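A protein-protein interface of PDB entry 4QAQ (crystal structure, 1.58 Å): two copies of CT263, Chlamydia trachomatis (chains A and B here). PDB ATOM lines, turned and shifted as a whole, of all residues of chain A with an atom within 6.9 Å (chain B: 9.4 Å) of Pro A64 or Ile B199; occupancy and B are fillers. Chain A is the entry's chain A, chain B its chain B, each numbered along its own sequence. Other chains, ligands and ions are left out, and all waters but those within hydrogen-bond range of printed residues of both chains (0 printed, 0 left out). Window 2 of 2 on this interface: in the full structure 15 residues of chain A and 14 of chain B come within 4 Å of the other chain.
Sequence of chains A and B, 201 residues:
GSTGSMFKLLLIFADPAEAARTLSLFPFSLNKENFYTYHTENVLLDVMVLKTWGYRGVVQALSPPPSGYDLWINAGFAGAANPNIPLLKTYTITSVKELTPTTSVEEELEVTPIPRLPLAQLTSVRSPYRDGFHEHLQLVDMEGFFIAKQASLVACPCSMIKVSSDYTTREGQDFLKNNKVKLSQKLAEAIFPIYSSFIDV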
ATOM      1  N   VAL A  59       9.666 -23.997   9.052  1.00  0.00           N
ATOM      2  CA  VAL A  59       9.819 -22.567   8.797  1.00  0.00           C
ATOM      3  C   VAL A  59       8.787 -22.093   7.785  1.00  0.00           C
ATOM      4  O   VAL A  59       8.338 -20.946   7.850  1.00  0.00           O
ATOM      5  CB  VAL A  59      11.250 -22.221   8.332  1.00  0.00           C
ATOM      6  CG1 VAL A  59      11.629 -22.997   7.071  1.00  0.00           C
ATOM      7  CG2 VAL A  59      11.378 -20.700   8.112  1.00  0.00           C
ATOM      8  N   GLN A  60       8.368 -22.962   6.861  1.00  0.00           N
ATOM      9  CA  GLN A  60       7.422 -22.536   5.826  1.00  0.00           C
ATOM     10  C   GLN A  60       5.996 -22.310   6.366  1.00  0.00           C
ATOM     11  O   GLN A  60       5.084 -21.994   5.588  1.00  0.00           O
ATOM     12  CB  GLN A  60       7.427 -23.551   4.684  1.00  0.00           C
ATOM     13  CG  GLN A  60       8.762 -23.556   3.947  1.00  0.00           C
ATOM     14  CD  GLN A  60       8.841 -24.586   2.834  1.00  0.00           C
ATOM     15  OE1 GLN A  60       9.683 -25.482   2.874  1.00  0.00           O
ATOM     16  NE2 GLN A  60       7.972 -24.450   1.820  1.00  0.00           N
ATOM     17  N   ALA A  61       5.766 -22.427   7.671  1.00  0.00           N
ATOM     18  CA  ALA A  61       4.480 -22.027   8.235  1.00  0.00           C
ATOM     19  C   ALA A  61       4.205 -20.536   8.056  1.00  0.00           C
ATOM     20  O   ALA A  61       3.040 -20.135   7.952  1.00  0.00           O
ATOM     21  CB  ALA A  61       4.420 -22.386   9.720  1.00  0.00           C
ATOM     22  N   LEU A  62       5.247 -19.693   8.062  1.00  0.00           N
ATOM     23  CA  LEU A  62       5.079 -18.244   7.918  1.00  0.00           C
ATOM     24  C   LEU A  62       6.127 -17.672   6.979  1.00  0.00           C
ATOM     25  O   LEU A  62       6.623 -16.562   7.192  1.00  0.00           O
ATOM     26  CB  LEU A  62       5.179 -17.516   9.275  1.00  0.00           C
ATOM     27  CG  LEU A  62       3.962 -17.335  10.164  1.00  0.00           C
ATOM     28  CD1 LEU A  62       4.399 -16.576  11.418  1.00  0.00           C
ATOM     29  CD2 LEU A  62       2.850 -16.603   9.477  1.00  0.00           C
ATOM     30  N   SER A  63       6.484 -18.419   5.946  1.00  0.00           N
ATOM     31  CA  SER A  63       7.552 -18.024   5.052  1.00  0.00           C
ATOM     32  C   SER A  63       7.100 -18.437   3.654  1.00  0.00           C
ATOM     33  O   SER A  63       6.956 -19.631   3.397  1.00  0.00           O
ATOM     34  CB  SER A  63       8.877 -18.684   5.433  1.00  0.00           C
ATOM     35  OG  SER A  63       9.892 -18.412   4.485  1.00  0.00           O
ATOM     36  N   PRO A  64       6.843 -17.464   2.756  1.00  0.00           N
ATOM     37  CA  PRO A  64       6.958 -16.016   2.962  1.00  0.00           C
ATOM     38  C   PRO A  64       5.896 -15.515   3.924  1.00  0.00           C
ATOM     39  O   PRO A  64       4.812 -16.101   3.976  1.00  0.00           O
ATOM     40  CB  PRO A  64       6.742 -15.437   1.566  1.00  0.00           C
ATOM     41  CG  PRO A  64       5.909 -16.446   0.878  1.00  0.00           C
ATOM     42  CD  PRO A  64       6.330 -17.781   1.412  1.00  0.00           C
ATOM     43  N   PRO A  65       6.209 -14.471   4.693  1.00  0.00           N
ATOM     44  CA  PRO A  65       5.250 -13.987   5.679  1.00  0.00           C
ATOM     45  C   PRO A  65       4.019 -13.417   5.002  1.00  0.00           C
ATOM     46  O   PRO A  65       4.110 -12.809   3.923  1.00  0.00           O
ATOM     47  CB  PRO A  65       6.036 -12.899   6.435  1.00  0.00           C
ATOM     48  CG  PRO A  65       7.165 -12.566   5.587  1.00  0.00           C
ATOM     49  CD  PRO A  65       7.499 -13.774   4.800  1.00  0.00           C
ATOM     50  N   PRO A  66       2.835 -13.597   5.597  1.00  0.00           N
ATOM     51  CA  PRO A  66       1.629 -12.965   5.053  1.00  0.00           C
ATOM     52  C   PRO A  66       1.760 -11.451   4.984  1.00  0.00           C
ATOM     53  O   PRO A  66       2.098 -10.789   5.962  1.00  0.00           O
ATOM     54  CB  PRO A  66       0.543 -13.391   6.048  1.00  0.00           C
ATOM     55  CG  PRO A  66       1.030 -14.638   6.628  1.00  0.00           C
ATOM     56  CD  PRO A  66       2.519 -14.477   6.730  1.00  0.00           C
ATOM     57  N   SER A  67       1.478 -10.897   3.816  1.00  0.00           N
ATOM     58  CA  SER A  67       1.478  -9.454   3.650  1.00  0.00           C
ATOM     59  C   SER A  67       0.053  -8.922   3.754  1.00  0.00           C
ATOM     60  O   SER A  67      -0.935  -9.665   3.662  1.00  0.00           O
ATOM     61  CB  SER A  67       2.082  -9.071   2.301  1.00  0.00           C
ATOM     62  OG  SER A  67       1.335  -9.680   1.266  1.00  0.00           O
ATOM     63  N   GLN A 150       9.347 -12.738  11.710  1.00  0.00           N
ATOM     64  CA  GLN A 150       8.666 -12.765  10.413  1.00  0.00           C
ATOM     65  C   GLN A 150       7.821 -11.510  10.224  1.00  0.00           C
ATOM     66  O   GLN A 150       7.728 -10.973   9.108  1.00  0.00           O
ATOM     67  CB  GLN A 150       7.817 -14.034  10.274  1.00  0.00           C
ATOM     68  CG  GLN A 150       8.616 -15.341  10.191  1.00  0.00           C
ATOM     69  CD  GLN A 150       9.686 -15.318   9.111  1.00  0.00           C
ATOM     70  OE1 GLN A 150      10.849 -15.037   9.392  1.00  0.00           O
ATOM     71  NE2 GLN A 150       9.292 -15.618   7.867  1.00  0.00           N
ATOM     72  N   LEU A 153       9.582  -8.676   8.656  1.00  0.00           N
ATOM     73  CA  LEU A 153       9.892  -8.768   7.231  1.00  0.00           C
ATOM     74  C   LEU A 153       8.860  -8.042   6.372  1.00  0.00           C
ATOM     75  O   LEU A 153       9.184  -7.584   5.267  1.00  0.00           O
ATOM     76  CB  LEU A 153      10.000 -10.229   6.797  1.00  0.00           C
ATOM     77  CG  LEU A 153      11.211 -11.018   7.307  1.00  0.00           C
ATOM     78  CD1 LEU A 153      11.174 -12.431   6.757  1.00  0.00           C
ATOM     79  CD2 LEU A 153      12.520 -10.356   6.932  1.00  0.00           C
ATOM     80  N   VAL A 154       7.627  -7.930   6.856  1.00  0.00           N
ATOM     81  CA  VAL A 154       6.570  -7.198   6.173  1.00  0.00           C
ATOM     82  C   VAL A 154       6.243  -5.899   6.894  1.00  0.00           C
ATOM     83  O   VAL A 154       5.220  -5.268   6.596  1.00  0.00           O
ATOM     84  CB  VAL A 154       5.313  -8.067   6.001  1.00  0.00           C
ATOM     85  CG1 VAL A 154       5.564  -9.153   4.973  1.00  0.00           C
ATOM     86  CG2 VAL A 154       4.891  -8.663   7.322  1.00  0.00           C
ATOM     87  N   MET B   6      12.336 -10.044  -9.614  1.00  0.00           N
ATOM     88  CA  MET B   6      13.072 -11.300  -9.313  1.00  0.00           C
ATOM     89  C   MET B   6      14.059 -11.124  -8.170  1.00  0.00           C
ATOM     90  O   MET B   6      14.994 -10.321  -8.236  1.00  0.00           O
ATOM     91  CB  MET B   6      13.828 -11.801 -10.544  1.00  0.00           C
ATOM     92  CG  MET B   6      12.971 -12.556 -11.525  1.00  0.00           C
ATOM     93  SD  MET B   6      13.912 -13.181 -12.921  1.00  0.00           S
ATOM     94  CE  MET B   6      14.681 -14.605 -12.174  1.00  0.00           C
ATOM     95  N   PHE B   7      13.842 -11.884  -7.112  1.00  0.00           N
ATOM     96  CA  PHE B   7      14.849 -11.989  -6.075  1.00  0.00           C
ATOM     97  C   PHE B   7      16.028 -12.780  -6.628  1.00  0.00           C
ATOM     98  O   PHE B   7      15.846 -13.765  -7.352  1.00  0.00           O
ATOM     99  CB  PHE B   7      14.268 -12.669  -4.835  1.00  0.00           C
ATOM    100  CG  PHE B   7      15.090 -12.471  -3.595  1.00  0.00           C
ATOM    101  CD1 PHE B   7      14.942 -11.329  -2.826  1.00  0.00           C
ATOM    102  CD2 PHE B   7      16.012 -13.427  -3.198  1.00  0.00           C
ATOM    103  CE1 PHE B   7      15.698 -11.147  -1.684  1.00  0.00           C
ATOM    104  CE2 PHE B   7      16.771 -13.251  -2.059  1.00  0.00           C
ATOM    105  CZ  PHE B   7      16.616 -12.110  -1.300  1.00  0.00           C
ATOM    106  N   LEU B   9      19.485 -14.756  -5.515  1.00  0.00           N
ATOM    107  CA  LEU B   9      20.153 -15.412  -4.400  1.00  0.00           C
ATOM    108  C   LEU B   9      21.437 -16.065  -4.892  1.00  0.00           C
ATOM    109  O   LEU B   9      21.415 -16.820  -5.866  1.00  0.00           O
ATOM    110  CB  LEU B   9      19.203 -16.449  -3.792  1.00  0.00           C
ATOM    111  CG  LEU B   9      19.594 -17.234  -2.539  1.00  0.00           C
ATOM    112  CD1 LEU B   9      20.021 -16.303  -1.430  1.00  0.00           C
ATOM    113  CD2 LEU B   9      18.392 -18.078  -2.104  1.00  0.00           C
ATOM    114  N   PHE B  26      17.596 -28.933  -7.266  1.00  0.00           N
ATOM    115  CA  PHE B  26      17.019 -28.202  -8.394  1.00  0.00           C
ATOM    116  C   PHE B  26      17.658 -28.645  -9.700  1.00  0.00           C
ATOM    117  O   PHE B  26      18.828 -29.035  -9.724  1.00  0.00           O
ATOM    118  CB  PHE B  26      17.241 -26.694  -8.253  1.00  0.00           C
ATOM    119  CG  PHE B  26      16.714 -26.101  -6.972  1.00  0.00           C
ATOM    120  CD1 PHE B  26      15.384 -25.698  -6.849  1.00  0.00           C
ATOM    121  CD2 PHE B  26      17.549 -25.965  -5.878  1.00  0.00           C
ATOM    122  CE1 PHE B  26      14.918 -25.159  -5.666  1.00  0.00           C
ATOM    123  CE2 PHE B  26      17.084 -25.407  -4.695  1.00  0.00           C
ATOM    124  CZ  PHE B  26      15.768 -25.015  -4.597  1.00  0.00           C
ATOM    125  N   TYR B  38      19.727 -21.596 -11.655  1.00  0.00           N
ATOM    126  CA  TYR B  38      18.335 -22.029 -11.728  1.00  0.00           C
ATOM    127  C   TYR B  38      17.406 -20.835 -11.558  1.00  0.00           C
ATOM    128  O   TYR B  38      17.633 -19.977 -10.704  1.00  0.00           O
ATOM    129  CB  TYR B  38      18.084 -23.049 -10.626  1.00  0.00           C
ATOM    130  CG  TYR B  38      16.664 -23.513 -10.565  1.00  0.00           C
ATOM    131  CD1 TYR B  38      16.144 -24.308 -11.547  1.00  0.00           C
ATOM    132  CD2 TYR B  38      15.838 -23.145  -9.496  1.00  0.00           C
ATOM    133  CE1 TYR B  38      14.804 -24.709 -11.494  1.00  0.00           C
ATOM    134  CE2 TYR B  38      14.547 -23.543  -9.433  1.00  0.00           C
ATOM    135  CZ  TYR B  38      14.040 -24.343 -10.414  1.00  0.00           C
ATOM    136  OH  TYR B  38      12.734 -24.730 -10.332  1.00  0.00           O
ATOM    137  N   HIS B  39      16.346 -20.765 -12.349  1.00  0.00           N
ATOM    138  CA  HIS B  39      15.412 -19.681 -12.117  1.00  0.00           C
ATOM    139  C   HIS B  39      13.977 -20.122 -12.326  1.00  0.00           C
ATOM    140  O   HIS B  39      13.679 -21.098 -13.016  1.00  0.00           O
ATOM    141  CB  HIS B  39      15.721 -18.484 -13.004  1.00  0.00           C
ATOM    142  CG  HIS B  39      15.360 -18.687 -14.437  1.00  0.00           C
ATOM    143  ND1 HIS B  39      16.244 -19.196 -15.361  1.00  0.00           N
ATOM    144  CD2 HIS B  39      14.212 -18.437 -15.112  1.00  0.00           C
ATOM    145  CE1 HIS B  39      15.654 -19.263 -16.541  1.00  0.00           C
ATOM    146  NE2 HIS B  39      14.420 -18.809 -16.418  1.00  0.00           N
ATOM    147  N   THR B  40      13.118 -19.443 -11.613  1.00  0.00           N
ATOM    148  CA  THR B  40      11.708 -19.380 -11.901  1.00  0.00           C
ATOM    149  C   THR B  40      11.399 -17.922 -12.180  1.00  0.00           C
ATOM    150  O   THR B  40      12.298 -17.068 -12.166  1.00  0.00           O
ATOM    151  CB  THR B  40      10.888 -19.894 -10.733  1.00  0.00           C
ATOM    152  OG1 THR B  40      11.089 -19.009  -9.625  1.00  0.00           O
ATOM    153  CG2 THR B  40      11.298 -21.317 -10.378  1.00  0.00           C
ATOM    154  N   GLU B  41      10.114 -17.633 -12.389  1.00  0.00           N
ATOM    155  CA  GLU B  41       9.715 -16.267 -12.692  1.00  0.00           C
ATOM    156  C   GLU B  41      10.079 -15.327 -11.556  1.00  0.00           C
ATOM    157  O   GLU B  41      10.405 -14.159 -11.798  1.00  0.00           O
ATOM    158  CB  GLU B  41       8.209 -16.207 -12.973  1.00  0.00           C
ATOM    159  N   ASN B  42      10.032 -15.810 -10.315  1.00  0.00           N
ATOM    160  CA  ASN B  42      10.196 -14.939  -9.156  1.00  0.00           C
ATOM    161  C   ASN B  42      11.598 -14.968  -8.552  1.00  0.00           C
ATOM    162  O   ASN B  42      11.963 -14.028  -7.844  1.00  0.00           O
ATOM    163  CB  ASN B  42       9.184 -15.316  -8.064  1.00  0.00           C
ATOM    164  N   VAL B  43      12.399 -15.991  -8.821  1.00  0.00           N
ATOM    165  CA  VAL B  43      13.623 -16.232  -8.058  1.00  0.00           C
ATOM    166  C   VAL B  43      14.723 -16.735  -8.983  1.00  0.00           C
ATOM    167  O   VAL B  43      14.539 -17.719  -9.703  1.00  0.00           O
ATOM    168  CB  VAL B  43      13.397 -17.264  -6.935  1.00  0.00           C
ATOM    169  CG1 VAL B  43      14.672 -17.417  -6.109  1.00  0.00           C
ATOM    170  CG2 VAL B  43      12.231 -16.870  -6.052  1.00  0.00           C
ATOM    171  N   LEU B  44      15.878 -16.080  -8.930  1.00  0.00           N
ATOM    172  CA  LEU B  44      17.117 -16.587  -9.506  1.00  0.00           C
ATOM    173  C   LEU B  44      17.976 -17.156  -8.387  1.00  0.00           C
ATOM    174  O   LEU B  44      18.193 -16.484  -7.369  1.00  0.00           O
ATOM    175  CB  LEU B  44      17.866 -15.470 -10.221  1.00  0.00           C
ATOM    176  CG  LEU B  44      19.299 -15.835 -10.639  1.00  0.00           C
ATOM    177  CD1 LEU B  44      19.254 -16.785 -11.821  1.00  0.00           C
ATOM    178  CD2 LEU B  44      20.099 -14.574 -10.964  1.00  0.00           C
ATOM    179  N   LEU B  45      18.395 -18.394  -8.548  1.00  0.00           N
ATOM    180  CA  LEU B  45      19.239 -19.091  -7.585  1.00  0.00           C
ATOM    181  C   LEU B  45      20.526 -19.488  -8.299  1.00  0.00           C
ATOM    182  O   LEU B  45      20.516 -20.379  -9.157  1.00  0.00           O
ATOM    183  CB  LEU B  45      18.513 -20.318  -7.029  1.00  0.00           C
ATOM    184  CG  LEU B  45      19.322 -21.155  -6.054  1.00  0.00           C
ATOM    185  CD1 LEU B  45      19.760 -20.321  -4.866  1.00  0.00           C
ATOM    186  CD2 LEU B  45      18.483 -22.373  -5.621  1.00  0.00           C
ATOM    187  N   PHE B 192      16.746 -25.363   1.173  1.00  0.00           N
ATOM    188  CA  PHE B 192      15.504 -25.487   0.407  1.00  0.00           C
ATOM    189  C   PHE B 192      14.436 -24.510   0.901  1.00  0.00           C
ATOM    190  O   PHE B 192      13.774 -23.867   0.067  1.00  0.00           O
ATOM    191  CB  PHE B 192      15.048 -26.962   0.460  1.00  0.00           C
ATOM    192  CG  PHE B 192      14.290 -27.493  -0.787  1.00  0.00           C
ATOM    193  CD1 PHE B 192      14.722 -27.247  -2.080  1.00  0.00           C
ATOM    194  CD2 PHE B 192      13.182 -28.327  -0.622  1.00  0.00           C
ATOM    195  CE1 PHE B 192      14.046 -27.766  -3.184  1.00  0.00           C
ATOM    196  CE2 PHE B 192      12.503 -28.848  -1.722  1.00  0.00           C
ATOM    197  CZ  PHE B 192      12.936 -28.563  -3.002  1.00  0.00           C
ATOM    198  N   PRO B 193      14.169 -24.396   2.207  1.00  0.00           N
ATOM    199  CA  PRO B 193      13.109 -23.475   2.637  1.00  0.00           C
ATOM    200  C   PRO B 193      13.457 -22.013   2.443  1.00  0.00           C
ATOM    201  O   PRO B 193      12.543 -21.194   2.282  1.00  0.00           O
ATOM    202  CB  PRO B 193      12.909 -23.818   4.118  1.00  0.00           C
ATOM    203  CG  PRO B 193      14.076 -24.599   4.519  1.00  0.00           C
ATOM    204  CD  PRO B 193      14.659 -25.242   3.314  1.00  0.00           C
ATOM    205  N   ILE B 194      14.737 -21.655   2.423  1.00  0.00           N
ATOM    206  CA  ILE B 194      15.121 -20.277   2.115  1.00  0.00           C
ATOM    207  C   ILE B 194      14.666 -19.924   0.710  1.00  0.00           C
ATOM    208  O   ILE B 194      14.054 -18.872   0.472  1.00  0.00           O
ATOM    209  CB  ILE B 194      16.637 -20.088   2.267  1.00  0.00           C
ATOM    210  CG1 ILE B 194      17.069 -20.432   3.694  1.00  0.00           C
ATOM    211  CG2 ILE B 194      17.031 -18.670   1.893  1.00  0.00           C
ATOM    212  CD1 ILE B 194      18.568 -20.367   3.912  1.00  0.00           C
ATOM    213  N   TYR B 195      14.935 -20.821  -0.236  1.00  0.00           N
ATOM    214  CA  TYR B 195      14.455 -20.634  -1.596  1.00  0.00           C
ATOM    215  C   TYR B 195      12.949 -20.416  -1.617  1.00  0.00           C
ATOM    216  O   TYR B 195      12.450 -19.493  -2.268  1.00  0.00           O
ATOM    217  CB  TYR B 195      14.840 -21.838  -2.466  1.00  0.00           C
ATOM    218  CG  TYR B 195      14.257 -21.778  -3.849  1.00  0.00           C
ATOM    219  CD1 TYR B 195      14.872 -21.030  -4.845  1.00  0.00           C
ATOM    220  CD2 TYR B 195      13.091 -22.451  -4.168  1.00  0.00           C
ATOM    221  CE1 TYR B 195      14.338 -20.944  -6.120  1.00  0.00           C
ATOM    222  CE2 TYR B 195      12.564 -22.385  -5.433  1.00  0.00           C
ATOM    223  CZ  TYR B 195      13.187 -21.617  -6.404  1.00  0.00           C
ATOM    224  OH  TYR B 195      12.682 -21.540  -7.674  1.00  0.00           O
ATOM    225  N   SER B 196      12.197 -21.250  -0.893  1.00  0.00           N
ATOM    226  CA  SER B 196      10.746 -21.086  -0.939  1.00  0.00           C
ATOM    227  C   SER B 196      10.288 -19.820  -0.219  1.00  0.00           C
ATOM    228  O   SER B 196       9.188 -19.345  -0.487  1.00  0.00           O
ATOM    229  CB  SER B 196      10.038 -22.313  -0.356  1.00  0.00           C
ATOM    230  OG  SER B 196      10.297 -22.453   1.028  1.00  0.00           O
ATOM    231  N   SER B 197      11.128 -19.229   0.639  1.00  0.00           N
ATOM    232  CA  SER B 197      10.773 -17.980   1.313  1.00  0.00           C
ATOM    233  C   SER B 197      10.639 -16.818   0.342  1.00  0.00           C
ATOM    234  O   SER B 197      10.122 -15.762   0.730  1.00  0.00           O
ATOM    235  CB  SER B 197      11.818 -17.640   2.394  1.00  0.00           C
ATOM    236  OG  SER B 197      13.006 -17.080   1.853  1.00  0.00           O
ATOM    237  N   PHE B 198      11.062 -16.996  -0.912  1.00  0.00           N
ATOM    238  CA  PHE B 198      11.022 -15.941  -1.916  1.00  0.00           C
ATOM    239  C   PHE B 198      10.033 -16.213  -3.037  1.00  0.00           C
ATOM    240  O   PHE B 198       9.866 -15.357  -3.913  1.00  0.00           O
ATOM    241  CB  PHE B 198      12.424 -15.735  -2.500  1.00  0.00           C
ATOM    242  CG  PHE B 198      13.436 -15.340  -1.474  1.00  0.00           C
ATOM    243  CD1 PHE B 198      13.328 -14.127  -0.820  1.00  0.00           C
ATOM    244  CD2 PHE B 198      14.476 -16.181  -1.143  1.00  0.00           C
ATOM    245  CE1 PHE B 198      14.243 -13.762   0.137  1.00  0.00           C
ATOM    246  CE2 PHE B 198      15.396 -15.819  -0.189  1.00  0.00           C
ATOM    247  CZ  PHE B 198      15.280 -14.612   0.453  1.00  0.00           C
ATOM    248  N   ILE B 199       9.364 -17.358  -3.036  1.00  0.00           N
ATOM    249  CA  ILE B 199       8.356 -17.639  -4.050  1.00  0.00           C
ATOM    250  C   ILE B 199       7.060 -16.892  -3.734  1.00  0.00           C
ATOM    251  O   ILE B 199       6.560 -16.951  -2.611  1.00  0.00           O
ATOM    252  CB  ILE B 199       8.084 -19.148  -4.156  1.00  0.00           C
ATOM    253  CG1 ILE B 199       9.351 -19.861  -4.631  1.00  0.00           C
ATOM    254  CG2 ILE B 199       6.926 -19.435  -5.116  1.00  0.00           C
ATOM    255  CD1 ILE B 199       9.272 -21.365  -4.545  1.00  0.00           C
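NE2 of Gln A60 sits close to OG of Ser B196 (3.2 Å).
The backbone carbonyl oxygen of Pro B193 sits at hydrogen-bond distance from the side-chain hydroxyl of Ser B196.
The backbone carbonyl oxygen (O) of Ile B194 is in hydrogen-bond range of the side-chain hydroxyl (OG) of Ser B197, at 2.5 Å.
Pro B193 touches Val A59 (CB to CG1, 3.3 Å).
Gln A60 touches Pro B193 (OE1 to CB, 3.8 Å).
OG of Ser A63 touches CB of Ser B197 (2.9 Å).
Pro A64 touches Ser B196 (CD to O, 3.8 Å).
Pro A64 touches Ser B197.
Ile B199 touches Pro A64.
Of the printed residues of chain B, Val A59 touches Pro B193.
Printed residues of chain B within 4 Å of Gln A60: Pro B193 (3.8 Å) and Ser B196 (3.2 Å).
Of chain B, only Ser B197 (2.9 Å) comes within 4 Å of Ser A63.
Of chain B, only Ser B196, Ser B197 and Ile B199 come within 4 Å of Pro A64.
Printed residues of chain A within 4 Å of Pro B193: Val A59 and Gln A60.
Ile B199 touches just one residue of chain A: Pro A64.
Printed residues of chain B that touch a printed residue of chain A: Pro B193, Ser B196, Ser B197 and Ile B199.
Along chain A the printed residues that touch a printed residue of chain B span positions 59 to 64.
Among the printed residues, no Asp or Glu carboxylate lies within 4 Å of a Lys or Arg side-chain nitrogen of the other chain.
No position is printed for both chains.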
